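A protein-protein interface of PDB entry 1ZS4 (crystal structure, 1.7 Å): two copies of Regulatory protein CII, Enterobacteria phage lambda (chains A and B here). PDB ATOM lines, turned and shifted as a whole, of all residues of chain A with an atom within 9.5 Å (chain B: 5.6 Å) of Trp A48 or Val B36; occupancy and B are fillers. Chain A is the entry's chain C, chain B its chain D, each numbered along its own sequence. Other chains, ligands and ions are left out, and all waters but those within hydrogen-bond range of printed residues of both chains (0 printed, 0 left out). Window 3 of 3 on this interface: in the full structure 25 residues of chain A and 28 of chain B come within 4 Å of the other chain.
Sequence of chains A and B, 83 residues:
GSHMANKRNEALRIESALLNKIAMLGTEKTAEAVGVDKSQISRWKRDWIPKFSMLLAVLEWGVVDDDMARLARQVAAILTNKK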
ATOM      1  N   ILE A  14      29.317 -15.817  25.312  1.00  0.00           N
ATOM      2  CA  ILE A  14      30.305 -16.228  24.312  1.00  0.00           C
ATOM      3  C   ILE A  14      29.974 -15.663  22.932  1.00  0.00           C
ATOM      4  O   ILE A  14      30.869 -15.208  22.211  1.00  0.00           O
ATOM      5  CB  ILE A  14      30.410 -17.769  24.230  1.00  0.00           C
ATOM      6  CG1 ILE A  14      31.067 -18.294  25.513  1.00  0.00           C
ATOM      7  CG2 ILE A  14      31.246 -18.200  22.994  1.00  0.00           C
ATOM      8  CD1 ILE A  14      31.004 -19.821  25.653  1.00  0.00           C
ATOM      9  N   GLU A  15      28.698 -15.693  22.554  1.00  0.00           N
ATOM     10  CA  GLU A  15      28.287 -15.158  21.256  1.00  0.00           C
ATOM     11  C   GLU A  15      28.626 -13.669  21.152  1.00  0.00           C
ATOM     12  O   GLU A  15      29.156 -13.197  20.141  1.00  0.00           O
ATOM     13  CB  GLU A  15      26.774 -15.330  21.062  1.00  0.00           C
ATOM     14  CG  GLU A  15      26.293 -14.852  19.688  1.00  0.00           C
ATOM     15  CD  GLU A  15      24.787 -14.957  19.531  1.00  0.00           C
ATOM     16  OE1 GLU A  15      24.159 -15.684  20.326  1.00  0.00           O
ATOM     17  OE2 GLU A  15      24.238 -14.320  18.604  1.00  0.00           O
ATOM     18  N   LEU A  18      32.374 -13.267  20.720  1.00  0.00           N
ATOM     19  CA  LEU A  18      32.819 -13.576  19.371  1.00  0.00           C
ATOM     20  C   LEU A  18      32.456 -12.452  18.404  1.00  0.00           C
ATOM     21  O   LEU A  18      33.296 -12.002  17.631  1.00  0.00           O
ATOM     22  CB  LEU A  18      32.198 -14.890  18.886  1.00  0.00           C
ATOM     23  CG  LEU A  18      32.826 -16.152  19.490  1.00  0.00           C
ATOM     24  CD1 LEU A  18      31.975 -17.361  19.133  1.00  0.00           C
ATOM     25  CD2 LEU A  18      34.262 -16.331  19.003  1.00  0.00           C
ATOM     26  N   LEU A  19      31.211 -12.000  18.461  1.00  0.00           N
ATOM     27  CA  LEU A  19      30.761 -10.934  17.570  1.00  0.00           C
ATOM     28  C   LEU A  19      31.516  -9.650  17.867  1.00  0.00           C
ATOM     29  O   LEU A  19      31.882  -8.915  16.953  1.00  0.00           O
ATOM     30  CB  LEU A  19      29.258 -10.697  17.733  1.00  0.00           C
ATOM     31  CG  LEU A  19      28.354 -11.843  17.283  1.00  0.00           C
ATOM     32  CD1 LEU A  19      26.887 -11.479  17.514  1.00  0.00           C
ATOM     33  CD2 LEU A  19      28.602 -12.128  15.815  1.00  0.00           C
ATOM     34  N   ILE A  22      35.105 -10.006  16.395  1.00  0.00           N
ATOM     35  CA  ILE A  22      35.096  -9.921  14.951  1.00  0.00           C
ATOM     36  C   ILE A  22      34.921  -8.456  14.553  1.00  0.00           C
ATOM     37  O   ILE A  22      35.629  -7.965  13.682  1.00  0.00           O
ATOM     38  CB  ILE A  22      33.940 -10.751  14.351  1.00  0.00           C
ATOM     39  CG1 ILE A  22      34.213 -12.241  14.590  1.00  0.00           C
ATOM     40  CG2 ILE A  22      33.797 -10.462  12.850  1.00  0.00           C
ATOM     41  CD1 ILE A  22      33.054 -13.139  14.209  1.00  0.00           C
ATOM     42  N   GLN A  40      31.584 -14.273   3.826  1.00  0.00           N
ATOM     43  CA  GLN A  40      31.487 -15.447   4.683  1.00  0.00           C
ATOM     44  C   GLN A  40      31.522 -15.059   6.156  1.00  0.00           C
ATOM     45  O   GLN A  40      30.762 -15.603   6.969  1.00  0.00           O
ATOM     46  CB  GLN A  40      32.609 -16.436   4.364  1.00  0.00           C
ATOM     47  CG  GLN A  40      32.368 -17.326   3.143  1.00  0.00           C
ATOM     48  CD  GLN A  40      31.300 -16.816   2.162  1.00  0.00           C
ATOM     49  OE1 GLN A  40      30.114 -17.114   2.299  1.00  0.00           O
ATOM     50  NE2 GLN A  40      31.520 -16.056   1.095  1.00  0.00           N
ATOM     51  N   ILE A  41      32.387 -14.112   6.520  1.00  0.00           N
ATOM     52  CA  ILE A  41      32.410 -13.729   7.935  1.00  0.00           C
ATOM     53  C   ILE A  41      31.051 -13.109   8.309  1.00  0.00           C
ATOM     54  O   ILE A  41      30.506 -13.377   9.381  1.00  0.00           O
ATOM     55  CB  ILE A  41      33.585 -12.766   8.248  1.00  0.00           C
ATOM     56  CG1 ILE A  41      34.913 -13.482   7.972  1.00  0.00           C
ATOM     57  CG2 ILE A  41      33.511 -12.302   9.714  1.00  0.00           C
ATOM     58  CD1 ILE A  41      35.125 -14.775   8.782  1.00  0.00           C
ATOM     59  N   SER A  42      30.481 -12.335   7.398  1.00  0.00           N
ATOM     60  CA  SER A  42      29.185 -11.721   7.663  1.00  0.00           C
ATOM     61  C   SER A  42      28.112 -12.771   7.828  1.00  0.00           C
ATOM     62  O   SER A  42      27.265 -12.671   8.721  1.00  0.00           O
ATOM     63  CB  SER A  42      28.688 -10.840   6.545  1.00  0.00           C
ATOM     64  OG  SER A  42      27.284 -10.689   6.593  1.00  0.00           O
ATOM     65  N   ARG A  43      28.152 -13.776   6.962  1.00  0.00           N
ATOM     66  CA  ARG A  43      27.181 -14.856   7.036  1.00  0.00           C
ATOM     67  C   ARG A  43      27.383 -15.807   8.222  1.00  0.00           C
ATOM     68  O   ARG A  43      26.397 -16.272   8.809  1.00  0.00           O
ATOM     69  CB  ARG A  43      27.138 -15.601   5.679  1.00  0.00           C
ATOM     70  CG  ARG A  43      26.484 -14.698   4.593  1.00  0.00           C
ATOM     71  CD  ARG A  43      26.377 -15.257   3.146  1.00  0.00           C
ATOM     72  NE  ARG A  43      25.257 -14.603   2.444  1.00  0.00           N
ATOM     73  CZ  ARG A  43      25.297 -14.052   1.223  1.00  0.00           C
ATOM     74  NH1 ARG A  43      26.420 -14.053   0.509  1.00  0.00           N
ATOM     75  NH2 ARG A  43      24.196 -13.477   0.720  1.00  0.00           N
ATOM     76  N   TRP A  44      28.634 -16.069   8.604  1.00  0.00           N
ATOM     77  CA  TRP A  44      28.888 -16.946   9.741  1.00  0.00           C
ATOM     78  C   TRP A  44      28.315 -16.333  11.010  1.00  0.00           C
ATOM     79  O   TRP A  44      27.839 -17.051  11.885  1.00  0.00           O
ATOM     80  CB  TRP A  44      30.380 -17.179   9.955  1.00  0.00           C
ATOM     81  CG  TRP A  44      31.052 -17.986   8.896  1.00  0.00           C
ATOM     82  CD1 TRP A  44      30.496 -18.502   7.751  1.00  0.00           C
ATOM     83  CD2 TRP A  44      32.433 -18.342   8.870  1.00  0.00           C
ATOM     84  NE1 TRP A  44      31.472 -19.153   7.010  1.00  0.00           N
ATOM     85  CE2 TRP A  44      32.664 -19.067   7.680  1.00  0.00           C
ATOM     86  CE3 TRP A  44      33.505 -18.112   9.742  1.00  0.00           C
ATOM     87  CZ2 TRP A  44      33.933 -19.569   7.341  1.00  0.00           C
ATOM     88  CZ3 TRP A  44      34.761 -18.610   9.407  1.00  0.00           C
ATOM     89  CH2 TRP A  44      34.966 -19.332   8.215  1.00  0.00           C
ATOM     90  N   LYS A  45      28.372 -15.011  11.110  1.00  0.00           N
ATOM     91  CA  LYS A  45      27.851 -14.330  12.286  1.00  0.00           C
ATOM     92  C   LYS A  45      26.371 -14.596  12.464  1.00  0.00           C
ATOM     93  O   LYS A  45      25.889 -14.801  13.575  1.00  0.00           O
ATOM     94  CB  LYS A  45      28.090 -12.821  12.183  1.00  0.00           C
ATOM     95  CG  LYS A  45      29.549 -12.424  12.305  1.00  0.00           C
ATOM     96  CD  LYS A  45      29.748 -10.911  12.352  1.00  0.00           C
ATOM     97  CE  LYS A  45      29.449 -10.260  11.025  1.00  0.00           C
ATOM     98  NZ  LYS A  45      29.903  -8.832  10.993  1.00  0.00           N
ATOM     99  N   ARG A  46      25.649 -14.620  11.357  1.00  0.00           N
ATOM    100  CA  ARG A  46      24.217 -14.822  11.408  1.00  0.00           C
ATOM    101  C   ARG A  46      23.775 -16.270  11.472  1.00  0.00           C
ATOM    102  O   ARG A  46      22.814 -16.599  12.172  1.00  0.00           O
ATOM    103  CB  ARG A  46      23.579 -14.124  10.207  1.00  0.00           C
ATOM    104  CG  ARG A  46      22.114 -14.442   9.993  1.00  0.00           C
ATOM    105  CD  ARG A  46      21.931 -15.208   8.692  1.00  0.00           C
ATOM    106  NE  ARG A  46      22.194 -14.384   7.514  1.00  0.00           N
ATOM    107  CZ  ARG A  46      22.520 -14.870   6.317  1.00  0.00           C
ATOM    108  NH1 ARG A  46      22.633 -16.182   6.133  1.00  0.00           N
ATOM    109  NH2 ARG A  46      22.720 -14.046   5.297  1.00  0.00           N
ATOM    110  N   ASP A  47      24.493 -17.142  10.776  1.00  0.00           N
ATOM    111  CA  ASP A  47      24.105 -18.536  10.713  1.00  0.00           C
ATOM    112  C   ASP A  47      24.626 -19.495  11.772  1.00  0.00           C
ATOM    113  O   ASP A  47      23.851 -20.105  12.502  1.00  0.00           O
ATOM    114  CB  ASP A  47      24.453 -19.113   9.334  1.00  0.00           C
ATOM    115  CG  ASP A  47      23.783 -18.366   8.188  1.00  0.00           C
ATOM    116  OD1 ASP A  47      22.617 -17.936   8.340  1.00  0.00           O
ATOM    117  OD2 ASP A  47      24.422 -18.228   7.126  1.00  0.00           O
ATOM    118  N   TRP A  48      25.937 -19.626  11.865  1.00  0.00           N
ATOM    119  CA  TRP A  48      26.503 -20.593  12.784  1.00  0.00           C
ATOM    120  C   TRP A  48      27.147 -20.114  14.079  1.00  0.00           C
ATOM    121  O   TRP A  48      27.300 -20.901  15.008  1.00  0.00           O
ATOM    122  CB  TRP A  48      27.476 -21.487  12.007  1.00  0.00           C
ATOM    123  CG  TRP A  48      26.798 -22.297  10.921  1.00  0.00           C
ATOM    124  CD1 TRP A  48      26.861 -22.083   9.573  1.00  0.00           C
ATOM    125  CD2 TRP A  48      25.911 -23.406  11.108  1.00  0.00           C
ATOM    126  NE1 TRP A  48      26.064 -22.991   8.907  1.00  0.00           N
ATOM    127  CE2 TRP A  48      25.471 -23.814   9.828  1.00  0.00           C
ATOM    128  CE3 TRP A  48      25.442 -24.094  12.237  1.00  0.00           C
ATOM    129  CZ2 TRP A  48      24.583 -24.882   9.643  1.00  0.00           C
ATOM    130  CZ3 TRP A  48      24.559 -25.156  12.056  1.00  0.00           C
ATOM    131  CH2 TRP A  48      24.138 -25.540  10.767  1.00  0.00           C
ATOM    132  N   ILE A  49      27.535 -18.848  14.168  1.00  0.00           N
ATOM    133  CA  ILE A  49      28.164 -18.389  15.398  1.00  0.00           C
ATOM    134  C   ILE A  49      27.251 -18.498  16.629  1.00  0.00           C
ATOM    135  O   ILE A  49      27.708 -18.873  17.712  1.00  0.00           O
ATOM    136  CB  ILE A  49      28.759 -16.965  15.205  1.00  0.00           C
ATOM    137  CG1 ILE A  49      30.071 -17.110  14.417  1.00  0.00           C
ATOM    138  CG2 ILE A  49      28.975 -16.269  16.558  1.00  0.00           C
ATOM    139  CD1 ILE A  49      30.763 -15.827  14.051  1.00  0.00           C
ATOM    140  N   PRO A  50      25.951 -18.185  16.489  1.00  0.00           N
ATOM    141  CA  PRO A  50      25.084 -18.308  17.669  1.00  0.00           C
ATOM    142  C   PRO A  50      25.043 -19.766  18.175  1.00  0.00           C
ATOM    143  O   PRO A  50      25.155 -20.012  19.383  1.00  0.00           O
ATOM    144  CB  PRO A  50      23.731 -17.826  17.150  1.00  0.00           C
ATOM    145  CG  PRO A  50      24.144 -16.759  16.177  1.00  0.00           C
ATOM    146  CD  PRO A  50      25.279 -17.417  15.421  1.00  0.00           C
ATOM    147  N   LYS A  51      24.907 -20.717  17.249  1.00  0.00           N
ATOM    148  CA  LYS A  51      24.862 -22.143  17.607  1.00  0.00           C
ATOM    149  C   LYS A  51      26.209 -22.636  18.111  1.00  0.00           C
ATOM    150  O   LYS A  51      26.283 -23.418  19.067  1.00  0.00           O
ATOM    151  CB  LYS A  51      24.453 -23.014  16.409  1.00  0.00           C
ATOM    152  CG  LYS A  51      23.046 -22.788  15.884  1.00  0.00           C
ATOM    153  CD  LYS A  51      22.036 -22.637  17.006  1.00  0.00           C
ATOM    154  CE  LYS A  51      21.842 -23.917  17.812  1.00  0.00           C
ATOM    155  NZ  LYS A  51      22.193 -23.737  19.250  1.00  0.00           N
ATOM    156  N   PHE A  52      27.276 -22.188  17.456  1.00  0.00           N
ATOM    157  CA  PHE A  52      28.613 -22.588  17.869  1.00  0.00           C
ATOM    158  C   PHE A  52      28.884 -22.069  19.286  1.00  0.00           C
ATOM    159  O   PHE A  52      29.573 -22.729  20.061  1.00  0.00           O
ATOM    160  CB  PHE A  52      29.652 -22.050  16.881  1.00  0.00           C
ATOM    161  CG  PHE A  52      31.071 -22.448  17.202  1.00  0.00           C
ATOM    162  CD1 PHE A  52      31.455 -23.787  17.217  1.00  0.00           C
ATOM    163  CD2 PHE A  52      32.034 -21.472  17.450  1.00  0.00           C
ATOM    164  CE1 PHE A  52      32.782 -24.159  17.472  1.00  0.00           C
ATOM    165  CE2 PHE A  52      33.377 -21.830  17.705  1.00  0.00           C
ATOM    166  CZ  PHE A  52      33.749 -23.178  17.717  1.00  0.00           C
ATOM    167  N   SER A  53      28.315 -20.908  19.627  1.00  0.00           N
ATOM    168  CA  SER A  53      28.491 -20.326  20.955  1.00  0.00           C
ATOM    169  C   SER A  53      27.852 -21.197  22.027  1.00  0.00           C
ATOM    170  O   SER A  53      28.371 -21.278  23.143  1.00  0.00           O
ATOM    171  CB  SER A  53      27.903 -18.904  20.990  1.00  0.00           C
ATOM    172  OG  SER A  53      28.662 -18.049  20.153  1.00  0.00           O
ATOM    173  N   MET A  54      26.728 -21.840  21.710  1.00  0.00           N
ATOM    174  CA  MET A  54      26.115 -22.732  22.697  1.00  0.00           C
ATOM    175  C   MET A  54      27.019 -23.950  22.843  1.00  0.00           C
ATOM    176  O   MET A  54      27.223 -24.426  23.950  1.00  0.00           O
ATOM    177  CB  MET A  54      24.714 -23.186  22.289  1.00  0.00           C
ATOM    178  CG  MET A  54      24.098 -24.220  23.239  1.00  0.00           C
ATOM    179  SD  MET A  54      24.051 -23.833  25.039  1.00  0.00           S
ATOM    180  CE  MET A  54      22.450 -23.093  25.183  1.00  0.00           C
ATOM    181  N   LEU A  55      27.558 -24.468  21.740  1.00  0.00           N
ATOM    182  CA  LEU A  55      28.477 -25.608  21.858  1.00  0.00           C
ATOM    183  C   LEU A  55      29.676 -25.206  22.757  1.00  0.00           C
ATOM    184  O   LEU A  55      30.067 -25.941  23.668  1.00  0.00           O
ATOM    185  CB  LEU A  55      28.996 -26.040  20.475  1.00  0.00           C
ATOM    186  CG  LEU A  55      30.046 -27.160  20.524  1.00  0.00           C
ATOM    187  CD1 LEU A  55      29.442 -28.400  21.186  1.00  0.00           C
ATOM    188  CD2 LEU A  55      30.533 -27.499  19.093  1.00  0.00           C
ATOM    189  N   LEU A  56      30.261 -24.040  22.512  1.00  0.00           N
ATOM    190  CA  LEU A  56      31.394 -23.625  23.333  1.00  0.00           C
ATOM    191  C   LEU A  56      30.980 -23.511  24.802  1.00  0.00           C
ATOM    192  O   LEU A  56      31.767 -23.802  25.690  1.00  0.00           O
ATOM    193  CB  LEU A  56      31.981 -22.299  22.832  1.00  0.00           C
ATOM    194  CG  LEU A  56      32.694 -22.342  21.474  1.00  0.00           C
ATOM    195  CD1 LEU A  56      33.428 -21.005  21.283  1.00  0.00           C
ATOM    196  CD2 LEU A  56      33.700 -23.486  21.407  1.00  0.00           C
ATOM    197  N   ALA B  31      25.201 -32.570  18.852  1.00  0.00           N
ATOM    198  CA  ALA B  31      24.176 -32.246  17.867  1.00  0.00           C
ATOM    199  C   ALA B  31      23.129 -31.325  18.488  1.00  0.00           C
ATOM    200  O   ALA B  31      22.683 -30.369  17.853  1.00  0.00           O
ATOM    201  CB  ALA B  31      23.522 -33.530  17.348  1.00  0.00           C
ATOM    202  N   GLU B  32      22.750 -31.604  19.734  1.00  0.00           N
ATOM    203  CA  GLU B  32      21.755 -30.791  20.433  1.00  0.00           C
ATOM    204  C   GLU B  32      22.253 -29.363  20.650  1.00  0.00           C
ATOM    205  O   GLU B  32      21.491 -28.416  20.509  1.00  0.00           O
ATOM    206  CB  GLU B  32      21.409 -31.403  21.790  1.00  0.00           C
ATOM    207  CG  GLU B  32      20.414 -30.568  22.605  1.00  0.00           C
ATOM    208  CD  GLU B  32      20.355 -30.965  24.081  1.00  0.00           C
ATOM    209  OE1 GLU B  32      19.574 -30.335  24.834  1.00  0.00           O
ATOM    210  OE2 GLU B  32      21.089 -31.896  24.498  1.00  0.00           O
ATOM    211  N   VAL B  34      24.430 -27.578  18.809  1.00  0.00           N
ATOM    212  CA  VAL B  34      24.450 -26.756  17.600  1.00  0.00           C
ATOM    213  C   VAL B  34      23.180 -26.777  16.759  1.00  0.00           C
ATOM    214  O   VAL B  34      23.105 -26.102  15.737  1.00  0.00           O
ATOM    215  CB  VAL B  34      25.662 -27.081  16.697  1.00  0.00           C
ATOM    216  CG1 VAL B  34      26.953 -26.771  17.445  1.00  0.00           C
ATOM    217  CG2 VAL B  34      25.644 -28.521  16.278  1.00  0.00           C
ATOM    218  N   GLY B  35      22.186 -27.545  17.192  1.00  0.00           N
ATOM    219  CA  GLY B  35      20.925 -27.617  16.470  1.00  0.00           C
ATOM    220  C   GLY B  35      20.989 -28.360  15.141  1.00  0.00           C
ATOM    221  O   GLY B  35      20.261 -28.037  14.195  1.00  0.00           O
ATOM    222  N   VAL B  36      21.863 -29.356  15.059  1.00  0.00           N
ATOM    223  CA  VAL B  36      22.024 -30.149  13.841  1.00  0.00           C
ATOM    224  C   VAL B  36      21.536 -31.579  14.115  1.00  0.00           C
ATOM    225  O   VAL B  36      21.720 -32.104  15.221  1.00  0.00           O
ATOM    226  CB  VAL B  36      23.525 -30.165  13.401  1.00  0.00           C
ATOM    227  CG1 VAL B  36      23.753 -31.218  12.335  1.00  0.00           C
ATOM    228  CG2 VAL B  36      23.931 -28.779  12.848  1.00  0.00           C
ATOM    229  N   ASP B  37      20.895 -32.213  13.132  1.00  0.00           N
ATOM    230  CA  ASP B  37      20.408 -33.574  13.348  1.00  0.00           C
ATOM    231  C   ASP B  37      21.583 -34.499  13.625  1.00  0.00           C
ATOM    232  O   ASP B  37      22.656 -34.338  13.057  1.00  0.00           O
ATOM    233  CB  ASP B  37      19.624 -34.090  12.129  1.00  0.00           C
ATOM    234  CG  ASP B  37      18.886 -35.396  12.413  1.00  0.00           C
ATOM    235  OD1 ASP B  37      19.512 -36.479  12.407  1.00  0.00           O
ATOM    236  OD2 ASP B  37      17.661 -35.340  12.658  1.00  0.00           O
ATOM    237  N   LYS B  38      21.369 -35.481  14.493  1.00  0.00           N
ATOM    238  CA  LYS B  38      22.422 -36.414  14.846  1.00  0.00           C
ATOM    239  C   LYS B  38      23.032 -37.106  13.622  1.00  0.00           C
ATOM    240  O   LYS B  38      24.212 -37.441  13.623  1.00  0.00           O
ATOM    241  CB  LYS B  38      21.871 -37.460  15.829  1.00  0.00           C
ATOM    242  CG  LYS B  38      22.941 -38.145  16.671  1.00  0.00           C
ATOM    243  CD  LYS B  38      22.315 -39.129  17.660  1.00  0.00           C
ATOM    244  CE  LYS B  38      23.354 -39.703  18.620  1.00  0.00           C
ATOM    245  NZ  LYS B  38      22.766 -40.756  19.491  1.00  0.00           N
ATOM    246  N   GLN B  40      23.676 -35.807  10.837  1.00  0.00           N
ATOM    247  CA  GLN B  40      24.503 -34.868  10.088  1.00  0.00           C
ATOM    248  C   GLN B  40      25.663 -34.264  10.878  1.00  0.00           C
ATOM    249  O   GLN B  40      26.518 -33.589  10.298  1.00  0.00           O
ATOM    250  CB  GLN B  40      23.630 -33.707   9.588  1.00  0.00           C
ATOM    251  CG  GLN B  40      22.552 -34.083   8.583  1.00  0.00           C
ATOM    252  CD  GLN B  40      23.133 -34.507   7.249  1.00  0.00           C
ATOM    253  OE1 GLN B  40      24.202 -34.029   6.842  1.00  0.00           O
ATOM    254  NE2 GLN B  40      22.424 -35.394   6.546  1.00  0.00           N
ATOM    255  N   ILE B  41      25.696 -34.502  12.186  1.00  0.00           N
ATOM    256  CA  ILE B  41      26.720 -33.886  13.027  1.00  0.00           C
ATOM    257  C   ILE B  41      28.177 -34.258  12.701  1.00  0.00           C
ATOM    258  O   ILE B  41      29.060 -33.416  12.831  1.00  0.00           O
ATOM    259  CB  ILE B  41      26.390 -34.127  14.536  1.00  0.00           C
ATOM    260  CG1 ILE B  41      27.212 -33.180  15.426  1.00  0.00           C
ATOM    261  CG2 ILE B  41      26.685 -35.561  14.912  1.00  0.00           C
ATOM    262  CD1 ILE B  41      26.969 -31.687  15.152  1.00  0.00           C
ATOM    263  N   TRP B  44      29.015 -32.169   9.754  1.00  0.00           N
ATOM    264  CA  TRP B  44      29.048 -30.787  10.193  1.00  0.00           C
ATOM    265  C   TRP B  44      30.385 -30.499  10.867  1.00  0.00           C
ATOM    266  O   TRP B  44      31.036 -29.504  10.564  1.00  0.00           O
ATOM    267  CB  TRP B  44      27.906 -30.496  11.177  1.00  0.00           C
ATOM    268  CG  TRP B  44      27.808 -29.046  11.530  1.00  0.00           C
ATOM    269  CD1 TRP B  44      27.070 -28.090  10.884  1.00  0.00           C
ATOM    270  CD2 TRP B  44      28.509 -28.369  12.579  1.00  0.00           C
ATOM    271  NE1 TRP B  44      27.273 -26.858  11.471  1.00  0.00           N
ATOM    272  CE2 TRP B  44      28.150 -27.002  12.513  1.00  0.00           C
ATOM    273  CE3 TRP B  44      29.409 -28.785  13.573  1.00  0.00           C
ATOM    274  CZ2 TRP B  44      28.658 -26.044  13.404  1.00  0.00           C
ATOM    275  CZ3 TRP B  44      29.915 -27.832  14.462  1.00  0.00           C
ATOM    276  CH2 TRP B  44      29.537 -26.476  14.369  1.00  0.00           C
ATOM    277  N   TRP B  48      32.984 -27.701   9.649  1.00  0.00           N
ATOM    278  CA  TRP B  48      33.046 -26.483  10.448  1.00  0.00           C
ATOM    279  C   TRP B  48      34.090 -26.319  11.535  1.00  0.00           C
ATOM    280  O   TRP B  48      34.546 -25.219  11.764  1.00  0.00           O
ATOM    281  CB  TRP B  48      31.663 -26.181  11.037  1.00  0.00           C
ATOM    282  CG  TRP B  48      30.703 -25.763   9.979  1.00  0.00           C
ATOM    283  CD1 TRP B  48      29.762 -26.540   9.361  1.00  0.00           C
ATOM    284  CD2 TRP B  48      30.642 -24.483   9.357  1.00  0.00           C
ATOM    285  NE1 TRP B  48      29.120 -25.814   8.389  1.00  0.00           N
ATOM    286  CE2 TRP B  48      29.640 -24.548   8.365  1.00  0.00           C
ATOM    287  CE3 TRP B  48      31.340 -23.284   9.540  1.00  0.00           C
ATOM    288  CZ2 TRP B  48      29.315 -23.450   7.553  1.00  0.00           C
ATOM    289  CZ3 TRP B  48      31.021 -22.196   8.736  1.00  0.00           C
ATOM    290  CH2 TRP B  48      30.013 -22.291   7.753  1.00  0.00           C
ATOM    291  N   PHE B  52      36.100 -22.872  12.205  1.00  0.00           N
ATOM    292  CA  PHE B  52      35.999 -22.143  13.447  1.00  0.00           C
ATOM    293  C   PHE B  52      37.305 -22.209  14.248  1.00  0.00           C
ATOM    294  O   PHE B  52      37.575 -21.302  15.022  1.00  0.00           O
ATOM    295  CB  PHE B  52      34.822 -22.664  14.275  1.00  0.00           C
ATOM    296  CG  PHE B  52      33.479 -22.331  13.692  1.00  0.00           C
ATOM    297  CD1 PHE B  52      32.405 -23.195  13.853  1.00  0.00           C
ATOM    298  CD2 PHE B  52      33.283 -21.136  13.005  1.00  0.00           C
ATOM    299  CE1 PHE B  52      31.140 -22.877  13.339  1.00  0.00           C
ATOM    300  CE2 PHE B  52      32.021 -20.807  12.488  1.00  0.00           C
ATOM    301  CZ  PHE B  52      30.953 -21.686  12.661  1.00  0.00           C
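The backbone carbonyl oxygen (O) of Trp A44 sits at hydrogen-bond distance from the backbone NH (N) of Ile A49 (2.9 Å). The backbone carbonyl oxygen (O) of Ala B31 lies within hydrogen-bond range of the backbone NH (N) of Val B36 (3.1 Å).
Trp A44 touches Trp B48, and with the chains exchanged Trp A48 touches Trp B44. Trp A48 touches its own counterpart, Trp B48. Trp A48 touches Phe B52, but with the chains exchanged Phe A52 does not touch Trp B48 (6.1 Å). Phe A52 touches its own counterpart, Phe B52. Positions printed for both chains: 40, 41, 44, 48 and 52. Of the 9 pairs that touch across the chains among the printed residues, 4 have their exchanged pair printed and touching as well.
Of chain B, only Val B36, Trp B44, Trp B48 and Phe B52 come within 4 Å of Trp A48. Printed residues of chain B within 4 Å of Lys A51: Val B34 (3.3 Å) and Gly B35 (3.7 Å). Of the printed residues of chain B, Leu A55 touches Val B34 (3.7 Å). Ala B31 touches none of the printed residues of chain A. Of chain A, only Lys A51 comes within 4 Å of Gly B35. Val B36 touches one residue of chain A. Of the printed residues of chain A, Trp B44 touches Trp A48. Printed residues of chain A within 4 Å of Trp B48: Trp A44 and Trp A48. Printed residues of chain A within 4 Å of Phe B52: Trp A48 and Phe A52. The nearest residue of chain B that does not touch Trp A48 is Val B34 (4.1 Å).
Printed residues of chain A that touch a printed residue of chain B: Trp A44, Trp A48, Lys A51, Phe A52 and Leu A55. Hydrophobic or aromatic side chains of chain A that line the printed part of chain B: Trp A44, Trp A48, Phe A52 and Leu A55. Hydrophobic or aromatic side chains of chain B within 4 Å of the printed part of chain A: Val B34, Val B36, Trp B44, Trp B48 and Phe B52. Along chain B the printed residues that touch a printed residue of chain A span positions 34 to 52. Among the printed residues, no Asp or Glu carboxylate lies within 4 Å of a Lys or Arg side-chain nitrogen of the other chain.
Among the printed residues, merely in contact across the chains: Trp A44 with Trp B48, Trp A48 with Val B36, Trp A48 with Trp B44, Trp A48 with Trp B48, Trp A48 with Phe B52, Lys A51 with Val B34, Lys A51 with Gly B35, Phe A52 with Phe B52 and Leu A55 with Val B34.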
